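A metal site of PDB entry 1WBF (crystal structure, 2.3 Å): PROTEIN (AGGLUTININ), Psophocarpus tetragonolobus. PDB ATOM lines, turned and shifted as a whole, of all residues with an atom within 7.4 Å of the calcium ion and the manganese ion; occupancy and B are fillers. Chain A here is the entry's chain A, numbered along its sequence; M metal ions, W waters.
The guanidinium group of Arg 128 lies within hydrogen-bond range of the backbone carbonyl oxygen of Asp 132 (3.1 Å). ND1 of His 137 lies close to O of Pro 133 (3.2 Å). The side-chain carboxylate of Asp 141 lies close to the side-chain carboxylate of Glu 123. OE2 of Glu 123 sits close to OG of Ser 147, 3.4 Å away. The backbone carbonyl oxygen (O) of Glu 123 lies within hydrogen-bond range of the backbone NH (N) of Gly 139, at 2.8 Å. A ring nitrogen (NE2) of His 137 lies close to the side-chain carboxylate of Asp 132 (3.2 Å). O of His 137 is in hydrogen-bond range of N of Asp 125 (3.0 Å).
Of the 26 residues printed, 4 come within 4 Å of the calcium ion.
Of the 26 residues printed, 4 come within 4 Å of the manganese ion.
Water W2 binds the calcium ion, 2.3 Å away. OD2 of Asp 132 binds the calcium ion. The calcium ion is bound by O of Phe 127, 2.4 Å away. OD1 of Asp 125 is bound to the calcium ion (2.5 Å). The calcium ion is bound by OD1 of Asn 129. The calcium ion is bound by the side-chain carboxylate (OD2) of Asp 125 (2.7 Å). The calcium ion is bound by water W3, at 2.7 Å.
The manganese ion is bound by water W4 (2.2 Å), the side-chain carboxylate of Glu 123 (2.2 Å), the side-chain carboxylate of Asp 132 (2.3 Å), water W1 (2.4 Å) and the side-chain carboxylate of Asp 125 (2.6 Å). The manganese ion has five donor atoms within binding distance. Slightly farther from the manganese ion lies a ring nitrogen (NE2) of His 137 (2.9 Å).
Water W3 bridges O of Gly 106 (2.5 Å) and NE1 of Trp 131 (3.5 Å). Water W1 lies within hydrogen-bond range of NE2 of His 137 (2.9 Å) and OG of Ser 147 (3.0 Å). Water W4 lies within hydrogen-bond range of O of Val 145 (2.6 Å) and OE1 of Glu 123 (2.7 Å).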
ATOM      1  N   ASP A  88      19.512  10.743  12.088  1.00  0.00           N
ATOM      2  CA  ASP A  88      20.654   9.954  12.580  1.00  0.00           C
ATOM      3  C   ASP A  88      20.324   8.517  12.935  1.00  0.00           C
ATOM      4  O   ASP A  88      21.167   7.634  12.764  1.00  0.00           O
ATOM      5  CB  ASP A  88      21.278  10.626  13.808  1.00  0.00           C
ATOM      6  CG  ASP A  88      22.391  11.597  13.435  1.00  0.00           C
ATOM      7  OD1 ASP A  88      23.496  11.150  13.068  1.00  0.00           O
ATOM      8  OD2 ASP A  88      22.155  12.805  13.489  1.00  0.00           O
ATOM      9  N   GLY A  89      19.106   8.269  13.420  1.00  0.00           N
ATOM     10  CA  GLY A  89      18.686   6.918  13.756  1.00  0.00           C
ATOM     11  C   GLY A  89      17.827   6.873  15.011  1.00  0.00           C
ATOM     12  O   GLY A  89      17.519   7.921  15.578  1.00  0.00           O
ATOM     13  N   GLY A 105      21.881  14.071  17.426  1.00  0.00           N
ATOM     14  CA  GLY A 105      22.801  13.620  16.406  1.00  0.00           C
ATOM     15  C   GLY A 105      23.129  12.146  16.526  1.00  0.00           C
ATOM     16  O   GLY A 105      22.248  11.313  16.749  1.00  0.00           O
ATOM     17  N   GLY A 106      24.412  11.819  16.396  1.00  0.00           N
ATOM     18  CA  GLY A 106      24.854  10.432  16.495  1.00  0.00           C
ATOM     19  C   GLY A 106      24.809   9.860  17.901  1.00  0.00           C
ATOM     20  O   GLY A 106      25.356   8.796  18.115  1.00  0.00           O
ATOM     21  N   TYR A 107      24.233  10.604  18.854  1.00  0.00           N
ATOM     22  CA  TYR A 107      24.083  10.158  20.249  1.00  0.00           C
ATOM     23  C   TYR A 107      22.650   9.743  20.522  1.00  0.00           C
ATOM     24  O   TYR A 107      22.332   9.302  21.630  1.00  0.00           O
ATOM     25  CB  TYR A 107      24.441  11.276  21.230  1.00  0.00           C
ATOM     26  CG  TYR A 107      25.913  11.629  21.270  1.00  0.00           C
ATOM     27  CD1 TYR A 107      26.872  10.762  20.766  1.00  0.00           C
ATOM     28  CD2 TYR A 107      26.328  12.842  21.796  1.00  0.00           C
ATOM     29  CE1 TYR A 107      28.218  11.102  20.770  1.00  0.00           C
ATOM     30  CE2 TYR A 107      27.674  13.192  21.803  1.00  0.00           C
ATOM     31  CZ  TYR A 107      28.604  12.315  21.295  1.00  0.00           C
ATOM     32  OH  TYR A 107      29.943  12.654  21.306  1.00  0.00           O
ATOM     33  N   PHE A 108      21.761  10.046  19.563  1.00  0.00           N
ATOM     34  CA  PHE A 108      20.342   9.658  19.632  1.00  0.00           C
ATOM     35  C   PHE A 108      19.492  10.264  20.733  1.00  0.00           C
ATOM     36  O   PHE A 108      18.338   9.859  20.923  1.00  0.00           O
ATOM     37  CB  PHE A 108      20.233   8.121  19.709  1.00  0.00           C
ATOM     38  CG  PHE A 108      21.107   7.385  18.724  1.00  0.00           C
ATOM     39  CD1 PHE A 108      20.866   7.455  17.353  1.00  0.00           C
ATOM     40  CD2 PHE A 108      22.208   6.658  19.171  1.00  0.00           C
ATOM     41  CE1 PHE A 108      21.710   6.814  16.447  1.00  0.00           C
ATOM     42  CE2 PHE A 108      23.059   6.015  18.272  1.00  0.00           C
ATOM     43  CZ  PHE A 108      22.810   6.093  16.910  1.00  0.00           C
ATOM     44  N   GLU A 123      20.576  -0.023  18.665  1.00  0.00           N
ATOM     45  CA  GLU A 123      20.454   1.051  17.704  1.00  0.00           C
ATOM     46  C   GLU A 123      20.297   0.627  16.250  1.00  0.00           C
ATOM     47  O   GLU A 123      20.914  -0.338  15.814  1.00  0.00           O
ATOM     48  CB  GLU A 123      21.695   1.961  17.771  1.00  0.00           C
ATOM     49  CG  GLU A 123      22.944   1.244  17.289  1.00  0.00           C
ATOM     50  CD  GLU A 123      24.167   2.123  17.225  1.00  0.00           C
ATOM     51  OE1 GLU A 123      24.425   2.888  18.179  1.00  0.00           O
ATOM     52  OE2 GLU A 123      24.882   1.993  16.237  1.00  0.00           O
ATOM     53  N   PHE A 124      19.524   1.412  15.515  1.00  0.00           N
ATOM     54  CA  PHE A 124      19.290   1.227  14.092  1.00  0.00           C
ATOM     55  C   PHE A 124      19.778   2.579  13.621  1.00  0.00           C
ATOM     56  O   PHE A 124      19.106   3.616  13.790  1.00  0.00           O
ATOM     57  CB  PHE A 124      17.797   0.977  13.829  1.00  0.00           C
ATOM     58  CG  PHE A 124      17.259  -0.211  14.568  1.00  0.00           C
ATOM     59  CD1 PHE A 124      17.332  -1.490  14.021  1.00  0.00           C
ATOM     60  CD2 PHE A 124      16.726  -0.056  15.851  1.00  0.00           C
ATOM     61  CE1 PHE A 124      16.874  -2.589  14.732  1.00  0.00           C
ATOM     62  CE2 PHE A 124      16.260  -1.151  16.585  1.00  0.00           C
ATOM     63  CZ  PHE A 124      16.334  -2.417  16.026  1.00  0.00           C
ATOM     64  N   ASP A 125      21.042   2.543  13.209  1.00  0.00           N
ATOM     65  CA  ASP A 125      21.853   3.685  12.802  1.00  0.00           C
ATOM     66  C   ASP A 125      21.955   3.938  11.309  1.00  0.00           C
ATOM     67  O   ASP A 125      22.483   3.117  10.555  1.00  0.00           O
ATOM     68  CB  ASP A 125      23.256   3.464  13.368  1.00  0.00           C
ATOM     69  CG  ASP A 125      24.043   4.750  13.537  1.00  0.00           C
ATOM     70  OD1 ASP A 125      24.168   5.510  12.562  1.00  0.00           O
ATOM     71  OD2 ASP A 125      24.535   4.986  14.653  1.00  0.00           O
ATOM     72  N   THR A 126      21.633   5.174  10.932  1.00  0.00           N
ATOM     73  CA  THR A 126      21.599   5.598   9.540  1.00  0.00           C
ATOM     74  C   THR A 126      22.657   6.585   9.097  1.00  0.00           C
ATOM     75  O   THR A 126      22.751   6.891   7.907  1.00  0.00           O
ATOM     76  CB  THR A 126      20.225   6.165   9.208  1.00  0.00           C
ATOM     77  OG1 THR A 126      19.944   7.269  10.071  1.00  0.00           O
ATOM     78  CG2 THR A 126      19.159   5.096   9.428  1.00  0.00           C
ATOM     79  N   PHE A 127      23.474   7.083  10.014  1.00  0.00           N
ATOM     80  CA  PHE A 127      24.516   8.041   9.651  1.00  0.00           C
ATOM     81  C   PHE A 127      25.894   7.534  10.078  1.00  0.00           C
ATOM     82  O   PHE A 127      26.084   7.136  11.226  1.00  0.00           O
ATOM     83  CB  PHE A 127      24.214   9.393  10.281  1.00  0.00           C
ATOM     84  CG  PHE A 127      25.193  10.454   9.918  1.00  0.00           C
ATOM     85  CD1 PHE A 127      25.425  10.780   8.599  1.00  0.00           C
ATOM     86  CD2 PHE A 127      25.860  11.149  10.913  1.00  0.00           C
ATOM     87  CE1 PHE A 127      26.317  11.783   8.263  1.00  0.00           C
ATOM     88  CE2 PHE A 127      26.744  12.147  10.597  1.00  0.00           C
ATOM     89  CZ  PHE A 127      26.977  12.476   9.265  1.00  0.00           C
ATOM     90  N   ARG A 128      26.869   7.519   9.175  1.00  0.00           N
ATOM     91  CA  ARG A 128      28.193   7.005   9.541  1.00  0.00           C
ATOM     92  C   ARG A 128      29.178   8.010  10.130  1.00  0.00           C
ATOM     93  O   ARG A 128      29.890   8.686   9.387  1.00  0.00           O
ATOM     94  CB  ARG A 128      28.868   6.301   8.375  1.00  0.00           C
ATOM     95  CG  ARG A 128      29.817   5.239   8.849  1.00  0.00           C
ATOM     96  CD  ARG A 128      31.159   5.393   8.236  1.00  0.00           C
ATOM     97  NE  ARG A 128      31.409   4.356   7.264  1.00  0.00           N
ATOM     98  CZ  ARG A 128      32.436   3.504   7.316  1.00  0.00           C
ATOM     99  NH1 ARG A 128      33.312   3.575   8.304  1.00  0.00           N
ATOM    100  NH2 ARG A 128      32.602   2.606   6.359  1.00  0.00           N
ATOM    101  N   ASN A 129      29.216   8.082  11.462  1.00  0.00           N
ATOM    102  CA  ASN A 129      30.147   8.956  12.173  1.00  0.00           C
ATOM    103  C   ASN A 129      31.533   8.348  12.104  1.00  0.00           C
ATOM    104  O   ASN A 129      31.713   7.271  11.570  1.00  0.00           O
ATOM    105  CB  ASN A 129      29.765   9.101  13.632  1.00  0.00           C
ATOM    106  CG  ASN A 129      28.461   9.773  13.819  1.00  0.00           C
ATOM    107  OD1 ASN A 129      27.426   9.136  13.771  1.00  0.00           O
ATOM    108  ND2 ASN A 129      28.495  11.064  14.097  1.00  0.00           N
ATOM    109  N   THR A 130      32.509   9.024  12.697  1.00  0.00           N
ATOM    110  CA  THR A 130      33.886   8.518  12.674  1.00  0.00           C
ATOM    111  C   THR A 130      34.034   7.202  13.442  1.00  0.00           C
ATOM    112  O   THR A 130      34.826   6.338  13.056  1.00  0.00           O
ATOM    113  CB  THR A 130      34.895   9.576  13.211  1.00  0.00           C
ATOM    114  OG1 THR A 130      34.435  10.084  14.476  1.00  0.00           O
ATOM    115  CG2 THR A 130      35.022  10.748  12.230  1.00  0.00           C
ATOM    116  N   TRP A 131      33.209   7.032  14.481  1.00  0.00           N
ATOM    117  CA  TRP A 131      33.234   5.842  15.324  1.00  0.00           C
ATOM    118  C   TRP A 131      32.259   4.766  14.864  1.00  0.00           C
ATOM    119  O   TRP A 131      31.885   3.897  15.646  1.00  0.00           O
ATOM    120  CB  TRP A 131      32.812   6.242  16.740  1.00  0.00           C
ATOM    121  CG  TRP A 131      31.383   6.714  16.819  1.00  0.00           C
ATOM    122  CD1 TRP A 131      30.250   5.954  16.724  1.00  0.00           C
ATOM    123  CD2 TRP A 131      30.959   8.061  17.030  1.00  0.00           C
ATOM    124  NE1 TRP A 131      29.146   6.739  16.871  1.00  0.00           N
ATOM    125  CE2 TRP A 131      29.537   8.041  17.061  1.00  0.00           C
ATOM    126  CE3 TRP A 131      31.605   9.276  17.193  1.00  0.00           C
ATOM    127  CZ2 TRP A 131      28.780   9.196  17.254  1.00  0.00           C
ATOM    128  CZ3 TRP A 131      30.855  10.430  17.393  1.00  0.00           C
ATOM    129  CH2 TRP A 131      29.453  10.369  17.422  1.00  0.00           C
ATOM    130  N   ASP A 132      31.837   4.839  13.611  1.00  0.00           N
ATOM    131  CA  ASP A 132      30.859   3.917  13.063  1.00  0.00           C
ATOM    132  C   ASP A 132      31.321   3.123  11.884  1.00  0.00           C
ATOM    133  O   ASP A 132      32.215   3.568  11.165  1.00  0.00           O
ATOM    134  CB  ASP A 132      29.668   4.702  12.546  1.00  0.00           C
ATOM    135  CG  ASP A 132      28.593   4.773  13.517  1.00  0.00           C
ATOM    136  OD1 ASP A 132      28.349   3.741  14.164  1.00  0.00           O
ATOM    137  OD2 ASP A 132      28.001   5.857  13.619  1.00  0.00           O
ATOM    138  N   PRO A 133      30.790   1.894  11.693  1.00  0.00           N
ATOM    139  CA  PRO A 133      31.117   1.018  10.556  1.00  0.00           C
ATOM    140  C   PRO A 133      30.068   1.358   9.477  1.00  0.00           C
ATOM    141  O   PRO A 133      29.145   2.117   9.740  1.00  0.00           O
ATOM    142  CB  PRO A 133      30.880  -0.387  11.125  1.00  0.00           C
ATOM    143  CG  PRO A 133      29.750  -0.182  12.052  1.00  0.00           C
ATOM    144  CD  PRO A 133      30.166   1.089  12.772  1.00  0.00           C
ATOM    145  N   ILE A 135      27.034   1.995   7.185  1.00  0.00           N
ATOM    146  CA  ILE A 135      25.603   2.123   7.511  1.00  0.00           C
ATOM    147  C   ILE A 135      24.688   1.649   6.356  1.00  0.00           C
ATOM    148  O   ILE A 135      25.139   1.546   5.207  1.00  0.00           O
ATOM    149  CB  ILE A 135      25.210   3.579   7.915  1.00  0.00           C
ATOM    150  CG1 ILE A 135      25.726   4.603   6.905  1.00  0.00           C
ATOM    151  CG2 ILE A 135      25.657   3.879   9.327  1.00  0.00           C
ATOM    152  CD1 ILE A 135      24.801   4.808   5.703  1.00  0.00           C
ATOM    153  N   HIS A 137      23.175  -0.045  10.034  1.00  0.00           N
ATOM    154  CA  HIS A 137      23.570  -1.202  10.825  1.00  0.00           C
ATOM    155  C   HIS A 137      22.866  -1.138  12.139  1.00  0.00           C
ATOM    156  O   HIS A 137      22.414  -0.065  12.555  1.00  0.00           O
ATOM    157  CB  HIS A 137      25.105  -1.274  11.059  1.00  0.00           C
ATOM    158  CG  HIS A 137      25.700  -0.061  11.721  1.00  0.00           C
ATOM    159  ND1 HIS A 137      26.628   0.752  11.096  1.00  0.00           N
ATOM    160  CD2 HIS A 137      25.510   0.474  12.957  1.00  0.00           C
ATOM    161  CE1 HIS A 137      26.984   1.735  11.908  1.00  0.00           C
ATOM    162  NE2 HIS A 137      26.312   1.584  13.043  1.00  0.00           N
ATOM    163  N   ILE A 138      22.637  -2.310  12.725  1.00  0.00           N
ATOM    164  CA  ILE A 138      22.024  -2.410  14.041  1.00  0.00           C
ATOM    165  C   ILE A 138      23.256  -2.504  14.943  1.00  0.00           C
ATOM    166  O   ILE A 138      24.284  -3.066  14.540  1.00  0.00           O
ATOM    167  CB  ILE A 138      21.282  -3.770  14.277  1.00  0.00           C
ATOM    168  CG1 ILE A 138      20.460  -4.197  13.056  1.00  0.00           C
ATOM    169  CG2 ILE A 138      20.403  -3.700  15.522  1.00  0.00           C
ATOM    170  CD1 ILE A 138      20.019  -5.692  13.125  1.00  0.00           C
ATOM    171  N   GLY A 139      23.159  -2.016  16.164  1.00  0.00           N
ATOM    172  CA  GLY A 139      24.284  -2.130  17.066  1.00  0.00           C
ATOM    173  C   GLY A 139      23.865  -2.289  18.504  1.00  0.00           C
ATOM    174  O   GLY A 139      22.816  -1.807  18.896  1.00  0.00           O
ATOM    175  N   ASP A 141      24.615  -1.303  22.234  1.00  0.00           N
ATOM    176  CA  ASP A 141      25.391  -0.295  22.941  1.00  0.00           C
ATOM    177  C   ASP A 141      25.338  -0.478  24.444  1.00  0.00           C
ATOM    178  O   ASP A 141      24.260  -0.609  25.004  1.00  0.00           O
ATOM    179  CB  ASP A 141      24.849   1.110  22.632  1.00  0.00           C
ATOM    180  CG  ASP A 141      24.894   1.438  21.170  1.00  0.00           C
ATOM    181  OD1 ASP A 141      25.648   0.772  20.458  1.00  0.00           O
ATOM    182  OD2 ASP A 141      24.197   2.376  20.748  1.00  0.00           O
ATOM    183  N   VAL A 145      28.052   4.864  22.401  1.00  0.00           N
ATOM    184  CA  VAL A 145      27.525   4.650  21.058  1.00  0.00           C
ATOM    185  C   VAL A 145      28.553   3.976  20.164  1.00  0.00           C
ATOM    186  O   VAL A 145      28.454   3.986  18.965  1.00  0.00           O
ATOM    187  CB  VAL A 145      27.015   5.941  20.353  1.00  0.00           C
ATOM    188  CG1 VAL A 145      25.745   6.433  21.015  1.00  0.00           C
ATOM    189  CG2 VAL A 145      28.081   7.019  20.359  1.00  0.00           C
ATOM    190  N   ILE A 146      29.615   3.452  20.751  1.00  0.00           N
ATOM    191  CA  ILE A 146      30.644   2.728  20.028  1.00  0.00           C
ATOM    192  C   ILE A 146      30.238   1.286  20.357  1.00  0.00           C
ATOM    193  O   ILE A 146      30.601   0.734  21.373  1.00  0.00           O
ATOM    194  CB  ILE A 146      32.046   3.076  20.529  1.00  0.00           C
ATOM    195  CG1 ILE A 146      32.186   4.609  20.605  1.00  0.00           C
ATOM    196  CG2 ILE A 146      33.097   2.510  19.567  1.00  0.00           C
ATOM    197  CD1 ILE A 146      33.433   5.123  21.322  1.00  0.00           C
ATOM    198  N   SER A 147      29.325   0.772  19.556  1.00  0.00           N
ATOM    199  CA  SER A 147      28.755  -0.566  19.701  1.00  0.00           C
ATOM    200  C   SER A 147      29.731  -1.680  19.997  1.00  0.00           C
ATOM    201  O   SER A 147      30.857  -1.699  19.468  1.00  0.00           O
ATOM    202  CB  SER A 147      27.949  -0.935  18.451  1.00  0.00           C
ATOM    203  OG  SER A 147      27.030   0.093  18.123  1.00  0.00           O
ATOM    204  N   THR A 150      28.019  -5.165  15.834  1.00  0.00           N
ATOM    205  CA  THR A 150      27.248  -4.526  14.752  1.00  0.00           C
ATOM    206  C   THR A 150      26.974  -5.488  13.585  1.00  0.00           C
ATOM    207  O   THR A 150      27.740  -6.431  13.362  1.00  0.00           O
ATOM    208  CB  THR A 150      27.868  -3.221  14.129  1.00  0.00           C
ATOM    209  OG1 THR A 150      29.022  -3.542  13.350  1.00  0.00           O
ATOM    210  CG2 THR A 150      28.196  -2.209  15.172  1.00  0.00           C
HETATM  211 CA    CA M   1      25.928   6.991  13.584  1.00  0.00          CA
HETATM  212 MN    MN M   2      26.409   3.349  15.313  1.00  0.00          MN
HETATM  213  O   HOH W   1      27.850   1.428  15.552  1.00  0.00           O
HETATM  214  O   HOH W   2      24.283   8.667  13.514  1.00  0.00           O
HETATM  215  O   HOH W   3      25.764   7.198  16.284  1.00  0.00           O
HETATM  216  O   HOH W   4      26.497   4.323  17.269  1.00  0.00           O
